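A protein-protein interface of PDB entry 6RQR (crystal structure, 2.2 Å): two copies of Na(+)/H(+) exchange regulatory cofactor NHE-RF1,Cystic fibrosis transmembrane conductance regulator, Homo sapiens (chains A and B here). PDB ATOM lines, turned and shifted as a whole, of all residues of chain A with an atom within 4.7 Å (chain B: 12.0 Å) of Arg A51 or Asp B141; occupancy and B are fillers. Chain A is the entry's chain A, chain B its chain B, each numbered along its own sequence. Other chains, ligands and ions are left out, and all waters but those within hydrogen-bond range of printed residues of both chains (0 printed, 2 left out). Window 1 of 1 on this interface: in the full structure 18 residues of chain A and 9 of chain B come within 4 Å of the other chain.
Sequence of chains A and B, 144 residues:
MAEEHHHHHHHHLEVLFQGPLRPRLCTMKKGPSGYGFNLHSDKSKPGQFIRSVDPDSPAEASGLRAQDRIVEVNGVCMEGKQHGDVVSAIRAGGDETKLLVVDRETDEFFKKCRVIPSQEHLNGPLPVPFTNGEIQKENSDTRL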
ATOM      1  N   ASN A  38      24.884  10.227   4.996  1.00  0.00           N
ATOM      2  CA  ASN A  38      25.204  10.237   6.417  1.00  0.00           C
ATOM      3  C   ASN A  38      24.732   8.942   7.060  1.00  0.00           C
ATOM      4  O   ASN A  38      23.581   8.535   6.875  1.00  0.00           O
ATOM      5  CB  ASN A  38      24.535  11.414   7.132  1.00  0.00           C
ATOM      6  CG  ASN A  38      25.005  12.756   6.621  1.00  0.00           C
ATOM      7  OD1 ASN A  38      24.575  13.207   5.561  1.00  0.00           O
ATOM      8  ND2 ASN A  38      25.898  13.401   7.362  1.00  0.00           N
ATOM      9  N   LEU A  39      25.619   8.307   7.816  1.00  0.00           N
ATOM     10  CA  LEU A  39      25.303   7.097   8.558  1.00  0.00           C
ATOM     11  C   LEU A  39      25.216   7.444  10.036  1.00  0.00           C
ATOM     12  O   LEU A  39      26.122   8.081  10.580  1.00  0.00           O
ATOM     13  CB  LEU A  39      26.365   6.025   8.325  1.00  0.00           C
ATOM     14  CG  LEU A  39      26.114   4.696   9.025  1.00  0.00           C
ATOM     15  CD1 LEU A  39      24.929   3.999   8.393  1.00  0.00           C
ATOM     16  CD2 LEU A  39      27.359   3.833   8.944  1.00  0.00           C
ATOM     17  N   HIS A  40      24.149   7.000  10.693  1.00  0.00           N
ATOM     18  CA  HIS A  40      23.911   7.361  12.083  1.00  0.00           C
ATOM     19  C   HIS A  40      23.565   6.127  12.900  1.00  0.00           C
ATOM     20  O   HIS A  40      22.934   5.192  12.404  1.00  0.00           O
ATOM     21  CB  HIS A  40      22.776   8.391  12.208  1.00  0.00           C
ATOM     22  CG  HIS A  40      22.390   8.702  13.621  1.00  0.00           C
ATOM     23  ND1 HIS A  40      23.109   9.569  14.416  1.00  0.00           N
ATOM     24  CD2 HIS A  40      21.359   8.265  14.382  1.00  0.00           C
ATOM     25  CE1 HIS A  40      22.538   9.651  15.605  1.00  0.00           C
ATOM     26  NE2 HIS A  40      21.474   8.869  15.611  1.00  0.00           N
ATOM     27  N   PHE A  49      21.892   3.384  10.382  1.00  0.00           N
ATOM     28  CA  PHE A  49      20.837   3.964   9.569  1.00  0.00           C
ATOM     29  C   PHE A  49      21.369   5.112   8.724  1.00  0.00           C
ATOM     30  O   PHE A  49      22.317   5.805   9.108  1.00  0.00           O
ATOM     31  CB  PHE A  49      19.685   4.457  10.449  1.00  0.00           C
ATOM     32  CG  PHE A  49      19.038   3.369  11.251  1.00  0.00           C
ATOM     33  CD1 PHE A  49      19.522   3.039  12.504  1.00  0.00           C
ATOM     34  CD2 PHE A  49      17.957   2.667  10.747  1.00  0.00           C
ATOM     35  CE1 PHE A  49      18.936   2.034  13.246  1.00  0.00           C
ATOM     36  CE2 PHE A  49      17.366   1.661  11.485  1.00  0.00           C
ATOM     37  CZ  PHE A  49      17.856   1.345  12.737  1.00  0.00           C
ATOM     38  N   ILE A  50      20.751   5.301   7.565  1.00  0.00           N
ATOM     39  CA  ILE A  50      21.073   6.414   6.683  1.00  0.00           C
ATOM     40  C   ILE A  50      20.259   7.611   7.155  1.00  0.00           C
ATOM     41  O   ILE A  50      19.041   7.657   6.973  1.00  0.00           O
ATOM     42  CB  ILE A  50      20.775   6.082   5.217  1.00  0.00           C
ATOM     43  CG1 ILE A  50      21.419   4.751   4.831  1.00  0.00           C
ATOM     44  CG2 ILE A  50      21.267   7.197   4.311  1.00  0.00           C
ATOM     45  CD1 ILE A  50      22.924   4.754   4.936  1.00  0.00           C
ATOM     46  N   ARG A  51      20.936   8.584   7.769  1.00  0.00           N
ATOM     47  CA  ARG A  51      20.237   9.770   8.248  1.00  0.00           C
ATOM     48  C   ARG A  51      19.913  10.716   7.101  1.00  0.00           C
ATOM     49  O   ARG A  51      18.842  11.336   7.082  1.00  0.00           O
ATOM     50  CB  ARG A  51      21.076  10.481   9.310  1.00  0.00           C
ATOM     51  CG  ARG A  51      20.619  11.901   9.609  1.00  0.00           C
ATOM     52  CD  ARG A  51      21.224  12.439  10.894  1.00  0.00           C
ATOM     53  NE  ARG A  51      20.545  11.918  12.077  1.00  0.00           N
ATOM     54  CZ  ARG A  51      20.859  12.253  13.325  1.00  0.00           C
ATOM     55  NH1 ARG A  51      21.847  13.108  13.554  1.00  0.00           N
ATOM     56  NH2 ARG A  51      20.186  11.734  14.342  1.00  0.00           N
ATOM     57  N   SER A  52      20.817  10.835   6.135  1.00  0.00           N
ATOM     58  CA  SER A  52      20.615  11.756   5.030  1.00  0.00           C
ATOM     59  C   SER A  52      21.408  11.274   3.827  1.00  0.00           C
ATOM     60  O   SER A  52      22.440  10.615   3.970  1.00  0.00           O
ATOM     61  CB  SER A  52      21.032  13.181   5.404  1.00  0.00           C
ATOM     62  OG  SER A  52      20.927  14.045   4.288  1.00  0.00           O
ATOM     63  N   VAL A  53      20.901  11.603   2.643  1.00  0.00           N
ATOM     64  CA  VAL A  53      21.602  11.374   1.387  1.00  0.00           C
ATOM     65  C   VAL A  53      21.562  12.673   0.594  1.00  0.00           C
ATOM     66  O   VAL A  53      20.497  13.280   0.441  1.00  0.00           O
ATOM     67  CB  VAL A  53      20.993  10.207   0.582  1.00  0.00           C
ATOM     68  CG1 VAL A  53      19.485  10.347   0.471  1.00  0.00           C
ATOM     69  CG2 VAL A  53      21.631  10.126  -0.794  1.00  0.00           C
ATOM     70  N   ALA A  66      17.011   8.046   2.869  1.00  0.00           N
ATOM     71  CA  ALA A  66      17.085   8.263   4.305  1.00  0.00           C
ATOM     72  C   ALA A  66      16.250   7.225   5.045  1.00  0.00           C
ATOM     73  O   ALA A  66      15.268   6.692   4.518  1.00  0.00           O
ATOM     74  CB  ALA A  66      16.606   9.671   4.658  1.00  0.00           C
ATOM     75  N   HIS A  83      29.364   0.689  15.037  1.00  0.00           N
ATOM     76  CA  HIS A  83      29.308   1.709  13.995  1.00  0.00           C
ATOM     77  C   HIS A  83      30.648   1.845  13.282  1.00  0.00           C
ATOM     78  O   HIS A  83      30.709   1.853  12.047  1.00  0.00           O
ATOM     79  CB  HIS A  83      28.883   3.044  14.606  1.00  0.00           C
ATOM     80  CG  HIS A  83      28.827   4.173  13.625  1.00  0.00           C
ATOM     81  ND1 HIS A  83      27.673   4.522  12.957  1.00  0.00           N
ATOM     82  CD2 HIS A  83      29.783   5.033  13.199  1.00  0.00           C
ATOM     83  CE1 HIS A  83      27.920   5.548  12.164  1.00  0.00           C
ATOM     84  NE2 HIS A  83      29.193   5.876  12.290  1.00  0.00           N
ATOM     85  N   ARG B 114      34.720  19.479  21.117  1.00  0.00           N
ATOM     86  CA  ARG B 114      35.152  18.392  20.237  1.00  0.00           C
ATOM     87  C   ARG B 114      35.614  18.941  18.892  1.00  0.00           C
ATOM     88  O   ARG B 114      35.316  18.392  17.829  1.00  0.00           O
ATOM     89  CB  ARG B 114      34.058  17.333  20.060  1.00  0.00           C
ATOM     90  CG  ARG B 114      33.838  16.427  21.273  1.00  0.00           C
ATOM     91  CD  ARG B 114      33.009  17.059  22.382  1.00  0.00           C
ATOM     92  NE  ARG B 114      33.350  16.481  23.682  1.00  0.00           N
ATOM     93  CZ  ARG B 114      32.848  15.346  24.161  1.00  0.00           C
ATOM     94  NH1 ARG B 114      31.968  14.651  23.452  1.00  0.00           N
ATOM     95  NH2 ARG B 114      33.227  14.903  25.352  1.00  0.00           N
ATOM     96  N   PHE B 130      29.462  20.927  23.396  1.00  0.00           N
ATOM     97  CA  PHE B 130      28.402  19.934  23.442  1.00  0.00           C
ATOM     98  C   PHE B 130      27.833  19.851  24.850  1.00  0.00           C
ATOM     99  O   PHE B 130      28.570  19.922  25.837  1.00  0.00           O
ATOM    100  CB  PHE B 130      28.937  18.564  23.024  1.00  0.00           C
ATOM    101  CG  PHE B 130      29.126  18.405  21.545  1.00  0.00           C
ATOM    102  CD1 PHE B 130      28.205  17.701  20.792  1.00  0.00           C
ATOM    103  CD2 PHE B 130      30.239  18.930  20.911  1.00  0.00           C
ATOM    104  CE1 PHE B 130      28.373  17.542  19.432  1.00  0.00           C
ATOM    105  CE2 PHE B 130      30.412  18.776  19.549  1.00  0.00           C
ATOM    106  CZ  PHE B 130      29.479  18.079  18.809  1.00  0.00           C
ATOM    107  N   GLY B 133      23.700  16.213  27.895  1.00  0.00           N
ATOM    108  CA  GLY B 133      22.581  15.427  27.404  1.00  0.00           C
ATOM    109  C   GLY B 133      22.773  14.959  25.977  1.00  0.00           C
ATOM    110  O   GLY B 133      22.317  13.874  25.607  1.00  0.00           O
ATOM    111  N   GLU B 134      23.451  15.763  25.157  1.00  0.00           N
ATOM    112  CA  GLU B 134      23.766  15.350  23.795  1.00  0.00           C
ATOM    113  C   GLU B 134      24.883  14.314  23.776  1.00  0.00           C
ATOM    114  O   GLU B 134      24.855  13.377  22.969  1.00  0.00           O
ATOM    115  CB  GLU B 134      24.139  16.575  22.958  1.00  0.00           C
ATOM    116  CG  GLU B 134      22.955  17.491  22.670  1.00  0.00           C
ATOM    117  CD  GLU B 134      23.369  18.829  22.095  1.00  0.00           C
ATOM    118  OE1 GLU B 134      24.440  19.340  22.484  1.00  0.00           O
ATOM    119  OE2 GLU B 134      22.629  19.368  21.245  1.00  0.00           O
ATOM    120  N   ILE B 135      25.879  14.475  24.652  1.00  0.00           N
ATOM    121  CA  ILE B 135      26.925  13.468  24.796  1.00  0.00           C
ATOM    122  C   ILE B 135      26.395  12.226  25.503  1.00  0.00           C
ATOM    123  O   ILE B 135      26.883  11.113  25.267  1.00  0.00           O
ATOM    124  CB  ILE B 135      28.126  14.077  25.543  1.00  0.00           C
ATOM    125  CG1 ILE B 135      28.521  15.406  24.900  1.00  0.00           C
ATOM    126  CG2 ILE B 135      29.306  13.123  25.563  1.00  0.00           C
ATOM    127  CD1 ILE B 135      29.634  16.114  25.613  1.00  0.00           C
ATOM    128  N   GLN B 136      25.383  12.383  26.363  1.00  0.00           N
ATOM    129  CA  GLN B 136      24.808  11.229  27.049  1.00  0.00           C
ATOM    130  C   GLN B 136      24.172  10.266  26.058  1.00  0.00           C
ATOM    131  O   GLN B 136      24.175   9.050  26.279  1.00  0.00           O
ATOM    132  CB  GLN B 136      23.817  11.709  28.110  1.00  0.00           C
ATOM    133  CG  GLN B 136      23.101  10.641  28.917  1.00  0.00           C
ATOM    134  CD  GLN B 136      22.039  11.256  29.812  1.00  0.00           C
ATOM    135  OE1 GLN B 136      21.814  12.467  29.769  1.00  0.00           O
ATOM    136  NE2 GLN B 136      21.396  10.435  30.637  1.00  0.00           N
ATOM    137  N   LYS B 137      23.618  10.793  24.964  1.00  0.00           N
ATOM    138  CA  LYS B 137      23.058   9.955  23.913  1.00  0.00           C
ATOM    139  C   LYS B 137      24.111   9.079  23.239  1.00  0.00           C
ATOM    140  O   LYS B 137      23.748   8.063  22.633  1.00  0.00           O
ATOM    141  CB  LYS B 137      22.365  10.824  22.867  1.00  0.00           C
ATOM    142  CG  LYS B 137      20.997  11.347  23.298  1.00  0.00           C
ATOM    143  CD  LYS B 137      19.970  10.229  23.277  1.00  0.00           C
ATOM    144  CE  LYS B 137      19.927   9.593  21.889  1.00  0.00           C
ATOM    145  NZ  LYS B 137      18.900   8.523  21.773  1.00  0.00           N
ATOM    146  N   GLU B 138      25.396   9.465  23.328  1.00  0.00           N
ATOM    147  CA  GLU B 138      26.539   8.777  22.696  1.00  0.00           C
ATOM    148  C   GLU B 138      26.324   8.592  21.197  1.00  0.00           C
ATOM    149  O   GLU B 138      26.547   7.509  20.649  1.00  0.00           O
ATOM    150  CB  GLU B 138      26.877   7.432  23.391  1.00  0.00           C
ATOM    151  CG  GLU B 138      25.920   6.222  23.242  1.00  0.00           C
ATOM    152  CD  GLU B 138      26.371   5.009  24.048  1.00  0.00           C
ATOM    153  OE1 GLU B 138      27.513   4.543  23.847  1.00  0.00           O
ATOM    154  OE2 GLU B 138      25.597   4.544  24.909  1.00  0.00           O
ATOM    155  N   ASN B 139      25.909   9.660  20.513  1.00  0.00           N
ATOM    156  CA  ASN B 139      25.629   9.531  19.088  1.00  0.00           C
ATOM    157  C   ASN B 139      26.916   9.299  18.308  1.00  0.00           C
ATOM    158  O   ASN B 139      27.981   9.809  18.668  1.00  0.00           O
ATOM    159  CB  ASN B 139      24.894  10.767  18.560  1.00  0.00           C
ATOM    160  CG  ASN B 139      23.478  10.866  19.080  1.00  0.00           C
ATOM    161  OD1 ASN B 139      22.747   9.879  19.078  1.00  0.00           O
ATOM    162  ND2 ASN B 139      23.083  12.047  19.524  1.00  0.00           N
ATOM    163  N   SER B 140      26.810   8.500  17.239  1.00  0.00           N
ATOM    164  CA  SER B 140      27.910   8.244  16.310  1.00  0.00           C
ATOM    165  C   SER B 140      27.422   8.525  14.900  1.00  0.00           C
ATOM    166  O   SER B 140      26.575   7.796  14.372  1.00  0.00           O
ATOM    167  CB  SER B 140      28.438   6.802  16.419  1.00  0.00           C
ATOM    168  OG  SER B 140      27.434   5.848  16.105  1.00  0.00           O
ATOM    169  N   ASP B 141      27.958   9.581  14.299  1.00  0.00           N
ATOM    170  CA  ASP B 141      27.593  10.016  12.962  1.00  0.00           C
ATOM    171  C   ASP B 141      28.849  10.051  12.102  1.00  0.00           C
ATOM    172  O   ASP B 141      29.944  10.334  12.591  1.00  0.00           O
ATOM    173  CB  ASP B 141      26.906  11.390  12.990  1.00  0.00           C
ATOM    174  CG  ASP B 141      25.571  11.353  13.717  1.00  0.00           C
ATOM    175  OD1 ASP B 141      25.574  11.325  14.965  1.00  0.00           O
ATOM    176  OD2 ASP B 141      24.520  11.338  13.043  1.00  0.00           O
ATOM    177  N   THR B 142      28.692   9.739  10.817  1.00  0.00           N
ATOM    178  CA  THR B 142      29.843   9.670   9.927  1.00  0.00           C
ATOM    179  C   THR B 142      29.453  10.181   8.552  1.00  0.00           C
ATOM    180  O   THR B 142      28.412   9.796   8.012  1.00  0.00           O
ATOM    181  CB  THR B 142      30.388   8.241   9.823  1.00  0.00           C
ATOM    182  OG1 THR B 142      30.748   7.768  11.125  1.00  0.00           O
ATOM    183  CG2 THR B 142      31.614   8.203   8.919  1.00  0.00           C
ATOM    184  N   ARG B 143      30.287  11.059   8.006  1.00  0.00           N
ATOM    185  CA  ARG B 143      30.118  11.564   6.652  1.00  0.00           C
ATOM    186  C   ARG B 143      30.775  10.600   5.675  1.00  0.00           C
ATOM    187  O   ARG B 143      31.973  10.318   5.781  1.00  0.00           O
ATOM    188  CB  ARG B 143      30.732  12.954   6.512  1.00  0.00           C
ATOM    189  CG  ARG B 143      30.872  13.397   5.077  1.00  0.00           C
ATOM    190  CD  ARG B 143      29.526  13.601   4.421  1.00  0.00           C
ATOM    191  NE  ARG B 143      29.675  13.915   3.004  1.00  0.00           N
ATOM    192  CZ  ARG B 143      28.668  14.207   2.189  1.00  0.00           C
ATOM    193  NH1 ARG B 143      27.427  14.252   2.650  1.00  0.00           N
ATOM    194  NH2 ARG B 143      28.905  14.473   0.911  1.00  0.00           N
ATOM    195  N   LEU B 144      29.990  10.092   4.731  1.00  0.00           N
ATOM    196  CA  LEU B 144      30.496   9.138   3.753  1.00  0.00           C
ATOM    197  C   LEU B 144      30.243   9.613   2.325  1.00  0.00           C
ATOM    198  O   LEU B 144      29.394  10.473   2.080  1.00  0.00           O
ATOM    199  CB  LEU B 144      29.862   7.766   3.977  1.00  0.00           C
ATOM    200  CG  LEU B 144      30.184   7.130   5.329  1.00  0.00           C
ATOM    201  CD1 LEU B 144      29.338   5.894   5.564  1.00  0.00           C
ATOM    202  CD2 LEU B 144      31.662   6.792   5.411  1.00  0.00           C
ATOM    203  OXT LEU B 144      30.881   9.142   1.381  1.00  0.00           O
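No position is printed for both chains. Of the 10 pairs that touch across the chains among the printed residues, none has its exchanged pair printed and touching as well.
The backbone carbonyl oxygen (O) of Asn A38 sits at hydrogen-bond distance from the backbone NH (N) of Arg A51 (2.8 Å). O of Ser A52 sits at hydrogen-bond distance from N of Asn A38, 2.7 Å away. N of His A40 lies within hydrogen-bond range of O of Phe A49, at 2.7 Å. NE2 of His A40 lies close to NH2 of Arg A51 (3.4 Å).
Asn A38 touches Thr B142 (CA to O, 3.6 Å). Ser B140 touches Leu A39. Asp B141 touches Leu A39 (CA to O, 3.4 Å). Asn B139 touches His A40. His A40 touches Ser B140 (CA to O, 3.5 Å).
Of the 14 printed residues of chain B, 4 touch a printed residue of chain A. Printed residues of chain B that touch a printed residue of chain A: Asn B139, Ser B140, Asp B141 and Thr B142. Printed residues of chain A that touch a printed residue of chain B: Asn A38, Leu A39, His A40, Arg A51 and His A83. Among the printed residues, 10 pairs touch across the chains. Among the printed residues, Asp or Glu carboxylates within 4 Å of a Lys or Arg side-chain nitrogen of the other chain: Arg A51 with Asp B141.
Of the printed residues of chain B, Arg A51 touches Asp B141 (3.2 Å). Asp B141 touches just these residues of chain A: Leu A39, His A40 and Arg A51. Of chain B, only Thr B142 comes within 4 Å of Asn A38. Of chain B, only Ser B140, Asp B141 and Thr B142 come within 4 Å of Leu A39. His A40 touches just these residues of chain B: Asn B139 (3.5 Å), Ser B140 (3.5 Å) and Asp B141 (2.6 Å). No residue of chain B comes within 4 Å of Ser A52. Of the printed residues of chain B, His A83 touches Ser B140 (3.3 Å) and Thr B142 (2.7 Å). Of the printed residues of chain A, Asn B139 touches His A40 (3.5 Å). Of the printed residues of chain A, Thr B142 touches Asn A38 (3.6 Å), Leu A39 (3.1 Å) and His A83 (2.7 Å). Gly B133 touches none of the printed residues of chain A. The nearest residue of chain B that does not touch Arg A51 is Asn B139 (5.7 Å).
The backbone NH (N) of Thr B142 lies within hydrogen-bond range of the backbone carbonyl oxygen (O) of Leu A39 (3.1 Å). OD2 of Asp B141 is in hydrogen-bond range of ND1 of His A40 (2.6 Å). The guanidinium group (NH1) of Arg A51 is in salt-bridge range of the side-chain carboxylate (OD2) of Asp B141, at 3.2 Å. ND1 of His A83 sits close to OG of Ser B140, 3.4 Å away. A ring nitrogen (NE2) of His A83 sits at hydrogen-bond distance from the side-chain hydroxyl of Thr B142, at 2.7 Å.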
